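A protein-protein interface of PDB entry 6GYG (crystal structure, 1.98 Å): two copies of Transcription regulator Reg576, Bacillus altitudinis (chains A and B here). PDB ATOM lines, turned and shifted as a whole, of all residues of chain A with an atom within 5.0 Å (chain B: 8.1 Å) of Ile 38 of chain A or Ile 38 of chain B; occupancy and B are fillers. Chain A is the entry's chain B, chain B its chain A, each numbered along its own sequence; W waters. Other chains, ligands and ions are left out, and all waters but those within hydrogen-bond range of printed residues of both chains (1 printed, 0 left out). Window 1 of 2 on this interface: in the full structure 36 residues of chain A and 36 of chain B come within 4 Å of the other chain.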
ATOM      1  N   LEU A  23      22.087 -14.285 -17.924  1.00  0.00           N
ATOM      2  CA  LEU A  23      23.297 -14.875 -18.492  1.00  0.00           C
ATOM      3  C   LEU A  23      24.147 -13.824 -19.206  1.00  0.00           C
ATOM      4  O   LEU A  23      25.349 -13.900 -19.103  1.00  0.00           O
ATOM      5  CB  LEU A  23      22.933 -16.019 -19.432  1.00  0.00           C
ATOM      6  CG  LEU A  23      24.080 -16.901 -19.905  1.00  0.00           C
ATOM      7  CD1 LEU A  23      24.821 -17.514 -18.744  1.00  0.00           C
ATOM      8  CD2 LEU A  23      23.537 -18.007 -20.823  1.00  0.00           C
ATOM      9  N   LEU A  34      25.443 -14.252 -27.554  1.00  0.00           N
ATOM     10  CA  LEU A  34      25.160 -15.197 -26.508  1.00  0.00           C
ATOM     11  C   LEU A  34      24.293 -16.326 -27.084  1.00  0.00           C
ATOM     12  O   LEU A  34      24.509 -17.500 -26.839  1.00  0.00           O
ATOM     13  CB  LEU A  34      24.482 -14.500 -25.324  1.00  0.00           C
ATOM     14  CG  LEU A  34      24.137 -15.388 -24.133  1.00  0.00           C
ATOM     15  CD1 LEU A  34      25.383 -16.091 -23.573  1.00  0.00           C
ATOM     16  CD2 LEU A  34      23.463 -14.598 -23.053  1.00  0.00           C
ATOM     17  N   ILE A  35      23.312 -15.971 -27.889  1.00  0.00           N
ATOM     18  CA  ILE A  35      22.464 -16.973 -28.489  1.00  0.00           C
ATOM     19  C   ILE A  35      23.274 -17.971 -29.310  1.00  0.00           C
ATOM     20  O   ILE A  35      23.026 -19.166 -29.270  1.00  0.00           O
ATOM     21  CB  ILE A  35      21.287 -16.327 -29.237  1.00  0.00           C
ATOM     22  CG1 ILE A  35      20.341 -15.750 -28.176  1.00  0.00           C
ATOM     23  CG2 ILE A  35      20.592 -17.349 -30.125  1.00  0.00           C
ATOM     24  CD1 ILE A  35      19.170 -15.053 -28.711  1.00  0.00           C
ATOM     25  N   GLU A  36      24.215 -17.472 -30.094  1.00  0.00           N
ATOM     26  CA  GLU A  36      25.002 -18.312 -30.902  1.00  0.00           C
ATOM     27  C   GLU A  36      25.823 -19.250 -30.035  1.00  0.00           C
ATOM     28  O   GLU A  36      25.919 -20.418 -30.318  1.00  0.00           O
ATOM     29  CB  GLU A  36      25.949 -17.475 -31.765  1.00  0.00           C
ATOM     30  CG  GLU A  36      26.601 -18.315 -32.858  1.00  0.00           C
ATOM     31  CD  GLU A  36      27.407 -17.548 -33.903  1.00  0.00           C
ATOM     32  OE1 GLU A  36      27.808 -16.377 -33.626  1.00  0.00           O
ATOM     33  OE2 GLU A  36      27.621 -18.120 -35.013  1.00  0.00           O
ATOM     34  N   ILE A  37      26.493 -18.698 -29.015  1.00  0.00           N
ATOM     35  CA  ILE A  37      27.348 -19.484 -28.113  1.00  0.00           C
ATOM     36  C   ILE A  37      26.562 -20.648 -27.478  1.00  0.00           C
ATOM     37  O   ILE A  37      27.026 -21.763 -27.441  1.00  0.00           O
ATOM     38  CB  ILE A  37      27.960 -18.541 -27.069  1.00  0.00           C
ATOM     39  CG1 ILE A  37      29.132 -17.797 -27.694  1.00  0.00           C
ATOM     40  CG2 ILE A  37      28.354 -19.284 -25.781  1.00  0.00           C
ATOM     41  CD1 ILE A  37      29.570 -16.658 -26.856  1.00  0.00           C
ATOM     42  N   ILE A  38      25.373 -20.383 -26.933  1.00  0.00           N
ATOM     43  CA  ILE A  38      24.586 -21.453 -26.317  1.00  0.00           C
ATOM     44  C   ILE A  38      24.000 -22.415 -27.385  1.00  0.00           C
ATOM     45  O   ILE A  38      23.835 -23.614 -27.086  1.00  0.00           O
ATOM     46  CB  ILE A  38      23.511 -20.899 -25.371  1.00  0.00           C
ATOM     47  CG1 ILE A  38      22.432 -20.116 -26.120  1.00  0.00           C
ATOM     48  CG2 ILE A  38      24.197 -20.052 -24.304  1.00  0.00           C
ATOM     49  CD1 ILE A  38      21.293 -19.707 -25.282  1.00  0.00           C
ATOM     50  N   LEU A  39      23.638 -21.935 -28.591  1.00  0.00           N
ATOM     51  CA  LEU A  39      23.294 -22.865 -29.668  1.00  0.00           C
ATOM     52  C   LEU A  39      24.445 -23.847 -29.941  1.00  0.00           C
ATOM     53  O   LEU A  39      24.227 -25.045 -29.975  1.00  0.00           O
ATOM     54  CB  LEU A  39      22.933 -22.127 -30.945  1.00  0.00           C
ATOM     55  CG  LEU A  39      21.517 -21.547 -30.949  1.00  0.00           C
ATOM     56  CD1 LEU A  39      21.358 -20.429 -31.977  1.00  0.00           C
ATOM     57  CD2 LEU A  39      20.537 -22.652 -31.250  1.00  0.00           C
ATOM     58  N   ASP A  40      25.630 -23.323 -30.214  1.00  0.00           N
ATOM     59  CA  ASP A  40      26.776 -24.134 -30.643  1.00  0.00           C
ATOM     60  C   ASP A  40      27.152 -25.146 -29.541  1.00  0.00           C
ATOM     61  O   ASP A  40      27.489 -26.286 -29.823  1.00  0.00           O
ATOM     62  CB  ASP A  40      27.959 -23.234 -30.999  1.00  0.00           C
ATOM     63  CG  ASP A  40      27.812 -22.421 -32.295  1.00  0.00           C
ATOM     64  OD1 ASP A  40      26.952 -22.781 -33.149  1.00  0.00           O
ATOM     65  OD2 ASP A  40      28.576 -21.431 -32.468  1.00  0.00           O
ATOM     66  N   PHE A  41      27.068 -24.725 -28.279  1.00  0.00           N
ATOM     67  CA  PHE A  41      27.427 -25.538 -27.145  1.00  0.00           C
ATOM     68  C   PHE A  41      26.461 -26.729 -27.096  1.00  0.00           C
ATOM     69  O   PHE A  41      26.875 -27.890 -26.827  1.00  0.00           O
ATOM     70  CB  PHE A  41      27.443 -24.712 -25.852  1.00  0.00           C
ATOM     71  CG  PHE A  41      27.914 -25.498 -24.655  1.00  0.00           C
ATOM     72  CD1 PHE A  41      29.261 -25.811 -24.490  1.00  0.00           C
ATOM     73  CD2 PHE A  41      27.023 -25.974 -23.720  1.00  0.00           C
ATOM     74  CE1 PHE A  41      29.695 -26.581 -23.420  1.00  0.00           C
ATOM     75  CE2 PHE A  41      27.462 -26.719 -22.646  1.00  0.00           C
ATOM     76  CZ  PHE A  41      28.788 -27.027 -22.502  1.00  0.00           C
ATOM     77  N   TYR A  42      25.178 -26.450 -27.349  1.00  0.00           N
ATOM     78  CA  TYR A  42      24.174 -27.511 -27.292  1.00  0.00           C
ATOM     79  C   TYR A  42      24.332 -28.476 -28.480  1.00  0.00           C
ATOM     80  O   TYR A  42      24.324 -29.693 -28.353  1.00  0.00           O
ATOM     81  CB  TYR A  42      22.784 -26.906 -27.361  1.00  0.00           C
ATOM     82  CG  TYR A  42      21.696 -27.892 -27.051  1.00  0.00           C
ATOM     83  CD1 TYR A  42      21.273 -28.104 -25.747  1.00  0.00           C
ATOM     84  CD2 TYR A  42      21.074 -28.581 -28.076  1.00  0.00           C
ATOM     85  CE1 TYR A  42      20.251 -28.989 -25.461  1.00  0.00           C
ATOM     86  CE2 TYR A  42      20.038 -29.443 -27.815  1.00  0.00           C
ATOM     87  CZ  TYR A  42      19.629 -29.648 -26.506  1.00  0.00           C
ATOM     88  OH  TYR A  42      18.652 -30.563 -26.281  1.00  0.00           O
ATOM     89  N   LYS B  19      20.743 -21.136 -37.697  1.00  0.00           N
ATOM     90  CA  LYS B  19      21.166 -22.260 -36.797  1.00  0.00           C
ATOM     91  C   LYS B  19      20.049 -22.584 -35.780  1.00  0.00           C
ATOM     92  O   LYS B  19      19.846 -23.752 -35.439  1.00  0.00           O
ATOM     93  CB  LYS B  19      22.436 -21.921 -36.031  1.00  0.00           C
ATOM     94  CG  LYS B  19      23.735 -21.877 -36.806  1.00  0.00           C
ATOM     95  CD  LYS B  19      24.925 -21.889 -35.839  1.00  0.00           C
ATOM     96  CE  LYS B  19      26.212 -21.390 -36.460  1.00  0.00           C
ATOM     97  NZ  LYS B  19      27.205 -20.972 -35.440  1.00  0.00           N
ATOM     98  N   LEU B  20      19.293 -21.559 -35.359  1.00  0.00           N
ATOM     99  CA  LEU B  20      18.119 -21.713 -34.461  1.00  0.00           C
ATOM    100  C   LEU B  20      16.972 -22.441 -35.167  1.00  0.00           C
ATOM    101  O   LEU B  20      16.310 -23.330 -34.565  1.00  0.00           O
ATOM    102  CB  LEU B  20      17.621 -20.350 -33.984  1.00  0.00           C
ATOM    103  CG  LEU B  20      16.304 -20.386 -33.201  1.00  0.00           C
ATOM    104  CD1 LEU B  20      16.499 -21.158 -31.920  1.00  0.00           C
ATOM    105  CD2 LEU B  20      15.799 -18.982 -32.893  1.00  0.00           C
ATOM    106  N   LEU B  23      17.953 -26.046 -35.619  1.00  0.00           N
ATOM    107  CA  LEU B  23      17.875 -26.857 -34.388  1.00  0.00           C
ATOM    108  C   LEU B  23      16.386 -27.064 -34.005  1.00  0.00           C
ATOM    109  O   LEU B  23      16.001 -28.068 -33.405  1.00  0.00           O
ATOM    110  CB  LEU B  23      18.668 -26.153 -33.291  1.00  0.00           C
ATOM    111  CG  LEU B  23      18.649 -26.856 -31.940  1.00  0.00           C
ATOM    112  CD1 LEU B  23      19.270 -28.239 -32.023  1.00  0.00           C
ATOM    113  CD2 LEU B  23      19.370 -26.020 -30.902  1.00  0.00           C
ATOM    114  N   LYS B  27      14.672 -30.856 -32.895  1.00  0.00           N
ATOM    115  CA  LYS B  27      13.850 -31.085 -31.738  1.00  0.00           C
ATOM    116  C   LYS B  27      12.388 -30.891 -32.163  1.00  0.00           C
ATOM    117  O   LYS B  27      12.014 -30.763 -33.366  1.00  0.00           O
ATOM    118  CB  LYS B  27      14.313 -30.105 -30.649  1.00  0.00           C
ATOM    119  CG  LYS B  27      15.787 -30.155 -30.332  1.00  0.00           C
ATOM    120  CD  LYS B  27      16.091 -31.119 -29.206  1.00  0.00           C
ATOM    121  CE  LYS B  27      17.316 -31.980 -29.436  1.00  0.00           C
ATOM    122  NZ  LYS B  27      17.283 -33.212 -28.605  1.00  0.00           N
ATOM    123  N   VAL B  29       9.961 -28.633 -30.614  1.00  0.00           N
ATOM    124  CA  VAL B  29       9.558 -27.721 -29.575  1.00  0.00           C
ATOM    125  C   VAL B  29       9.275 -26.351 -30.187  1.00  0.00           C
ATOM    126  O   VAL B  29       9.798 -26.042 -31.237  1.00  0.00           O
ATOM    127  CB  VAL B  29      10.605 -27.644 -28.441  1.00  0.00           C
ATOM    128  CG1 VAL B  29      10.733 -28.987 -27.733  1.00  0.00           C
ATOM    129  CG2 VAL B  29      11.953 -27.144 -28.937  1.00  0.00           C
ATOM    130  N   GLN B  31       9.849 -22.280 -30.415  1.00  0.00           N
ATOM    131  CA  GLN B  31      11.061 -21.513 -30.575  1.00  0.00           C
ATOM    132  C   GLN B  31      11.581 -20.993 -29.226  1.00  0.00           C
ATOM    133  O   GLN B  31      12.763 -21.206 -28.891  1.00  0.00           O
ATOM    134  CB  GLN B  31      10.769 -20.349 -31.507  1.00  0.00           C
ATOM    135  CG  GLN B  31      11.996 -19.606 -31.993  1.00  0.00           C
ATOM    136  CD  GLN B  31      11.526 -18.457 -32.848  1.00  0.00           C
ATOM    137  OE1 GLN B  31      10.965 -17.487 -32.344  1.00  0.00           O
ATOM    138  NE2 GLN B  31      11.725 -18.571 -34.150  1.00  0.00           N
ATOM    139  N   TYR B  32      10.718 -20.327 -28.451  1.00  0.00           N
ATOM    140  CA  TYR B  32      11.154 -19.836 -27.140  1.00  0.00           C
ATOM    141  C   TYR B  32      11.442 -21.029 -26.209  1.00  0.00           C
ATOM    142  O   TYR B  32      12.330 -20.883 -25.333  1.00  0.00           O
ATOM    143  CB  TYR B  32      10.221 -18.791 -26.518  1.00  0.00           C
ATOM    144  CG  TYR B  32       8.791 -19.237 -26.530  1.00  0.00           C
ATOM    145  CD1 TYR B  32       8.293 -20.085 -25.548  1.00  0.00           C
ATOM    146  CD2 TYR B  32       7.975 -18.913 -27.602  1.00  0.00           C
ATOM    147  CE1 TYR B  32       6.982 -20.540 -25.581  1.00  0.00           C
ATOM    148  CE2 TYR B  32       6.672 -19.374 -27.663  1.00  0.00           C
ATOM    149  CZ  TYR B  32       6.174 -20.184 -26.653  1.00  0.00           C
ATOM    150  OH  TYR B  32       4.876 -20.596 -26.739  1.00  0.00           O
ATOM    151  N   GLU B  33      10.775 -22.179 -26.382  1.00  0.00           N
ATOM    152  CA  GLU B  33      11.048 -23.370 -25.492  1.00  0.00           C
ATOM    153  C   GLU B  33      12.437 -23.957 -25.768  1.00  0.00           C
ATOM    154  O   GLU B  33      13.082 -24.578 -24.857  1.00  0.00           O
ATOM    155  CB  GLU B  33      10.042 -24.511 -25.681  1.00  0.00           C
ATOM    156  CG  GLU B  33       8.591 -24.084 -25.456  1.00  0.00           C
ATOM    157  CD  GLU B  33       7.493 -25.152 -25.552  1.00  0.00           C
ATOM    158  OE1 GLU B  33       7.473 -25.999 -26.522  1.00  0.00           O
ATOM    159  OE2 GLU B  33       6.658 -25.139 -24.636  1.00  0.00           O
ATOM    160  N   LEU B  34      12.867 -23.817 -27.034  1.00  0.00           N
ATOM    161  CA  LEU B  34      14.122 -24.300 -27.453  1.00  0.00           C
ATOM    162  C   LEU B  34      15.201 -23.455 -26.761  1.00  0.00           C
ATOM    163  O   LEU B  34      16.141 -23.999 -26.234  1.00  0.00           O
ATOM    164  CB  LEU B  34      14.272 -24.205 -28.974  1.00  0.00           C
ATOM    165  CG  LEU B  34      15.654 -24.607 -29.504  1.00  0.00           C
ATOM    166  CD1 LEU B  34      16.065 -26.026 -29.053  1.00  0.00           C
ATOM    167  CD2 LEU B  34      15.654 -24.530 -31.002  1.00  0.00           C
ATOM    168  N   ILE B  35      15.018 -22.122 -26.790  1.00  0.00           N
ATOM    169  CA  ILE B  35      15.946 -21.173 -26.189  1.00  0.00           C
ATOM    170  C   ILE B  35      16.117 -21.500 -24.701  1.00  0.00           C
ATOM    171  O   ILE B  35      17.256 -21.468 -24.203  1.00  0.00           O
ATOM    172  CB  ILE B  35      15.477 -19.719 -26.379  1.00  0.00           C
ATOM    173  CG1 ILE B  35      15.450 -19.299 -27.841  1.00  0.00           C
ATOM    174  CG2 ILE B  35      16.308 -18.757 -25.538  1.00  0.00           C
ATOM    175  CD1 ILE B  35      16.750 -19.481 -28.532  1.00  0.00           C
ATOM    176  N   GLU B  36      15.023 -21.830 -24.010  1.00  0.00           N
ATOM    177  CA  GLU B  36      15.104 -22.192 -22.603  1.00  0.00           C
ATOM    178  C   GLU B  36      15.904 -23.483 -22.361  1.00  0.00           C
ATOM    179  O   GLU B  36      16.696 -23.565 -21.414  1.00  0.00           O
ATOM    180  CB  GLU B  36      13.723 -22.369 -21.974  1.00  0.00           C
ATOM    181  CG  GLU B  36      13.820 -22.545 -20.475  1.00  0.00           C
ATOM    182  CD  GLU B  36      12.613 -22.100 -19.673  1.00  0.00           C
ATOM    183  OE1 GLU B  36      11.473 -22.236 -20.185  1.00  0.00           O
ATOM    184  OE2 GLU B  36      12.823 -21.629 -18.525  1.00  0.00           O
ATOM    185  N   ILE B  37      15.694 -24.497 -23.184  1.00  0.00           N
ATOM    186  CA  ILE B  37      16.438 -25.777 -23.083  1.00  0.00           C
ATOM    187  C   ILE B  37      17.940 -25.496 -23.251  1.00  0.00           C
ATOM    188  O   ILE B  37      18.755 -25.954 -22.497  1.00  0.00           O
ATOM    189  CB  ILE B  37      15.913 -26.772 -24.141  1.00  0.00           C
ATOM    190  CG1 ILE B  37      14.502 -27.247 -23.781  1.00  0.00           C
ATOM    191  CG2 ILE B  37      16.883 -27.949 -24.359  1.00  0.00           C
ATOM    192  CD1 ILE B  37      13.700 -27.736 -24.975  1.00  0.00           C
ATOM    193  N   ILE B  38      18.308 -24.693 -24.247  1.00  0.00           N
ATOM    194  CA  ILE B  38      19.706 -24.561 -24.497  1.00  0.00           C
ATOM    195  C   ILE B  38      20.373 -23.629 -23.465  1.00  0.00           C
ATOM    196  O   ILE B  38      21.536 -23.806 -23.169  1.00  0.00           O
ATOM    197  CB  ILE B  38      20.011 -24.126 -25.942  1.00  0.00           C
ATOM    198  CG1 ILE B  38      19.511 -22.736 -26.263  1.00  0.00           C
ATOM    199  CG2 ILE B  38      19.469 -25.132 -26.950  1.00  0.00           C
ATOM    200  CD1 ILE B  38      19.665 -22.420 -27.744  1.00  0.00           C
ATOM    201  N   LEU B  39      19.674 -22.575 -23.029  1.00  0.00           N
ATOM    202  CA  LEU B  39      20.063 -21.725 -21.912  1.00  0.00           C
ATOM    203  C   LEU B  39      20.353 -22.581 -20.681  1.00  0.00           C
ATOM    204  O   LEU B  39      21.360 -22.419 -20.054  1.00  0.00           O
ATOM    205  CB  LEU B  39      18.891 -20.791 -21.572  1.00  0.00           C
ATOM    206  CG  LEU B  39      18.924 -19.404 -22.200  1.00  0.00           C
ATOM    207  CD1 LEU B  39      17.648 -18.624 -21.867  1.00  0.00           C
ATOM    208  CD2 LEU B  39      20.128 -18.638 -21.714  1.00  0.00           C
ATOM    209  N   ASP B  40      19.383 -23.407 -20.291  1.00  0.00           N
ATOM    210  CA  ASP B  40      19.490 -24.271 -19.095  1.00  0.00           C
ATOM    211  C   ASP B  40      20.688 -25.223 -19.235  1.00  0.00           C
ATOM    212  O   ASP B  40      21.431 -25.427 -18.319  1.00  0.00           O
ATOM    213  CB  ASP B  40      18.226 -25.100 -18.884  1.00  0.00           C
ATOM    214  CG  ASP B  40      16.990 -24.338 -18.411  1.00  0.00           C
ATOM    215  OD1 ASP B  40      17.094 -23.105 -18.229  1.00  0.00           O
ATOM    216  OD2 ASP B  40      15.910 -24.995 -18.219  1.00  0.00           O
ATOM    217  N   PHE B  41      20.874 -25.785 -20.428  1.00  0.00           N
ATOM    218  CA  PHE B  41      21.945 -26.694 -20.639  1.00  0.00           C
ATOM    219  C   PHE B  41      23.291 -25.993 -20.497  1.00  0.00           C
ATOM    220  O   PHE B  41      24.275 -26.543 -19.897  1.00  0.00           O
ATOM    221  CB  PHE B  41      21.766 -27.395 -21.979  1.00  0.00           C
ATOM    222  CG  PHE B  41      22.856 -28.392 -22.244  1.00  0.00           C
ATOM    223  CD1 PHE B  41      22.836 -29.643 -21.622  1.00  0.00           C
ATOM    224  CD2 PHE B  41      23.911 -28.087 -23.098  1.00  0.00           C
ATOM    225  CE1 PHE B  41      23.832 -30.570 -21.894  1.00  0.00           C
ATOM    226  CE2 PHE B  41      24.909 -29.019 -23.343  1.00  0.00           C
ATOM    227  CZ  PHE B  41      24.836 -30.268 -22.786  1.00  0.00           C
ATOM    228  N   TYR B  42      23.340 -24.745 -20.943  1.00  0.00           N
ATOM    229  CA  TYR B  42      24.591 -23.980 -20.865  1.00  0.00           C
ATOM    230  C   TYR B  42      24.886 -23.581 -19.406  1.00  0.00           C
ATOM    231  O   TYR B  42      26.009 -23.671 -18.909  1.00  0.00           O
ATOM    232  CB  TYR B  42      24.524 -22.756 -21.772  1.00  0.00           C
ATOM    233  CG  TYR B  42      25.840 -22.047 -21.856  1.00  0.00           C
ATOM    234  CD1 TYR B  42      26.170 -21.074 -20.918  1.00  0.00           C
ATOM    235  CD2 TYR B  42      26.762 -22.332 -22.852  1.00  0.00           C
ATOM    236  CE1 TYR B  42      27.368 -20.380 -20.992  1.00  0.00           C
ATOM    237  CE2 TYR B  42      27.963 -21.644 -22.958  1.00  0.00           C
ATOM    238  CZ  TYR B  42      28.269 -20.674 -22.010  1.00  0.00           C
ATOM    239  OH  TYR B  42      29.456 -20.018 -22.003  1.00  0.00           O
ATOM    240  N   VAL B  43      23.859 -23.088 -18.709  1.00  0.00           N
ATOM    241  CA  VAL B  43      23.972 -22.723 -17.317  1.00  0.00           C
ATOM    242  C   VAL B  43      24.460 -23.927 -16.504  1.00  0.00           C
ATOM    243  O   VAL B  43      25.322 -23.778 -15.684  1.00  0.00           O
ATOM    244  CB  VAL B  43      22.647 -22.176 -16.786  1.00  0.00           C
ATOM    245  CG1 VAL B  43      22.614 -22.139 -15.258  1.00  0.00           C
ATOM    246  CG2 VAL B  43      22.340 -20.804 -17.391  1.00  0.00           C
ATOM    247  N   THR B  44      23.886 -25.106 -16.722  1.00  0.00           N
ATOM    248  CA  THR B  44      24.171 -26.290 -15.891  1.00  0.00           C
ATOM    249  C   THR B  44      25.548 -26.891 -16.172  1.00  0.00           C
ATOM    250  O   THR B  44      26.160 -27.478 -15.286  1.00  0.00           O
ATOM    251  CB  THR B  44      23.122 -27.367 -16.108  1.00  0.00           C
ATOM    252  OG1 THR B  44      22.025 -26.743 -15.465  1.00  0.00           O
ATOM    253  CG2 THR B  44      23.440 -28.702 -15.461  1.00  0.00           C
ATOM    254  N   ASN B  45      26.014 -26.791 -17.412  1.00  0.00           N
ATOM    255  CA  ASN B  45      27.130 -27.593 -17.839  1.00  0.00           C
ATOM    256  C   ASN B  45      28.319 -26.748 -18.262  1.00  0.00           C
ATOM    257  O   ASN B  45      29.358 -27.340 -18.581  1.00  0.00           O
ATOM    258  CB  ASN B  45      26.777 -28.515 -19.013  1.00  0.00           C
ATOM    259  CG  ASN B  45      25.746 -29.520 -18.595  1.00  0.00           C
ATOM    260  OD1 ASN B  45      26.068 -30.397 -17.825  1.00  0.00           O
ATOM    261  ND2 ASN B  45      24.496 -29.335 -18.992  1.00  0.00           N
ATOM    262  N   LYS B  46      28.184 -25.423 -18.315  1.00  0.00           N
ATOM    263  CA  LYS B  46      29.309 -24.625 -18.757  1.00  0.00           C
ATOM    264  C   LYS B  46      29.720 -23.536 -17.760  1.00  0.00           C
ATOM    265  O   LYS B  46      30.879 -23.228 -17.682  1.00  0.00           O
ATOM    266  CB  LYS B  46      29.015 -24.035 -20.128  1.00  0.00           C
ATOM    267  CG  LYS B  46      30.172 -23.289 -20.774  1.00  0.00           C
ATOM    268  CD  LYS B  46      31.399 -24.166 -20.890  1.00  0.00           C
ATOM    269  CE  LYS B  46      32.259 -23.794 -22.076  1.00  0.00           C
ATOM    270  NZ  LYS B  46      33.496 -24.600 -22.047  1.00  0.00           N
HETATM  271  O   HOH W   1      23.727 -24.723 -24.613  1.00  0.00           O
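Ile 37 of chain A touches Tyr 42 of chain B, and with the chains exchanged Tyr 42 of chain A touches Ile 37 of chain B. Ile 38 of chain B touches its own counterpart, Ile 38 of chain A. Ile 38 of chain A touches Leu 39 of chain B, and with the chains exchanged Leu 39 of chain A touches Ile 38 of chain B. Ile 38 of chain A touches Tyr 42 of chain B, and with the chains exchanged Tyr 42 of chain A touches Ile 38 of chain B. Positions printed for both chains: 23, 34, 35, 36, 37, 38, 39, 40, 41 and 42. Of the 17 pairs that touch across the chains among the printed residues, 12 have their exchanged pair printed and touching as well.
Water W1 bridges the backbone carbonyl oxygen of Ile 38 of chain A (2.7 Å) and the backbone carbonyl oxygen of Ile 38 of chain B (2.8 Å).
Ile 38 of chain A touches just these residues of chain B: Ile 38, Leu 39 and Tyr 42. Printed residues of chain A within 4 Å of Ile 38 of chain B: Ile 38, Leu 39 and Tyr 42. Of the printed residues of chain B, Leu 39 of chain A touches Leu 23 (3.6 Å) and Ile 38 (3.6 Å). Printed residues of chain B within 4 Å of Glu 36 of chain A: Lys 19. Thr 44 of chain B touches none of the printed residues of chain A. Val 43 of chain B touches none of the printed residues of chain A. The nearest residue of chain B that does not touch Ile 38 of chain A is Ile 35 of chain B (4.5 Å).
Among the printed residues, pairs that only touch across the chains: Leu 23 of chain A with Leu 39 of chain B (3.6 Å), Ile 37 of chain A with Tyr 42 of chain B (3.7 Å), Ile 38 of chain A with Ile 38 of chain B (3.6 Å), Ile 38 of chain A with Leu 39 of chain B (3.9 Å), Ile 38 of chain A with Tyr 42 of chain B (3.6 Å), Leu 39 of chain A with Leu 23 of chain B (3.6 Å), Leu 39 of chain A with Ile 38 of chain B (3.6 Å), Phe 41 of chain A with Phe 41 of chain B (3.5 Å), Phe 41 of chain A with Tyr 42 of chain B (3.8 Å), Phe 41 of chain A with Asn 45 of chain B (3.97 Å), Phe 41 of chain A with Lys 46 of chain B (3.8 Å), Tyr 42 of chain A with Lys 27 of chain B (3.7 Å), Tyr 42 of chain A with Ile 37 of chain B (3.7 Å), Tyr 42 of chain A with Ile 38 of chain B (3.5 Å) and Tyr 42 of chain A with Phe 41 of chain B (3.7 Å).
Hydrophobic or aromatic side chains of chain A that line the printed part of chain B: Leu 23, Ile 37, Ile 38, Leu 39, Phe 41 and Tyr 42. Of the 21 printed residues of chain B, 10 touch a printed residue of chain A. Hydrophobic or aromatic side chains of chain B within 4 Å of the printed part of chain A: Leu 23, Ile 37, Ile 38, Leu 39, Phe 41 and Tyr 42. Among the printed residues, Asp or Glu carboxylates within 4 Å of a Lys or Arg side-chain nitrogen of the other chain: Glu 36 of chain A with Lys 19 of chain B (2.9 Å) and Asp 40 of chain A with Lys 19 of chain B (2.9 Å).
ND2 of Asn 45 of chain B sits at hydrogen-bond distance from O of Phe 41 of chain B.
The side-chain amino group (NZ) of Lys 19 of chain B lies within salt-bridge range of the side-chain carboxylate (OD1) of Asp 40 of chain A (2.9 Å). The side-chain amino group (NZ) of Lys 19 of chain B is in salt-bridge range of the side-chain carboxylate (OE2) of Glu 36 of chain A (2.9 Å).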
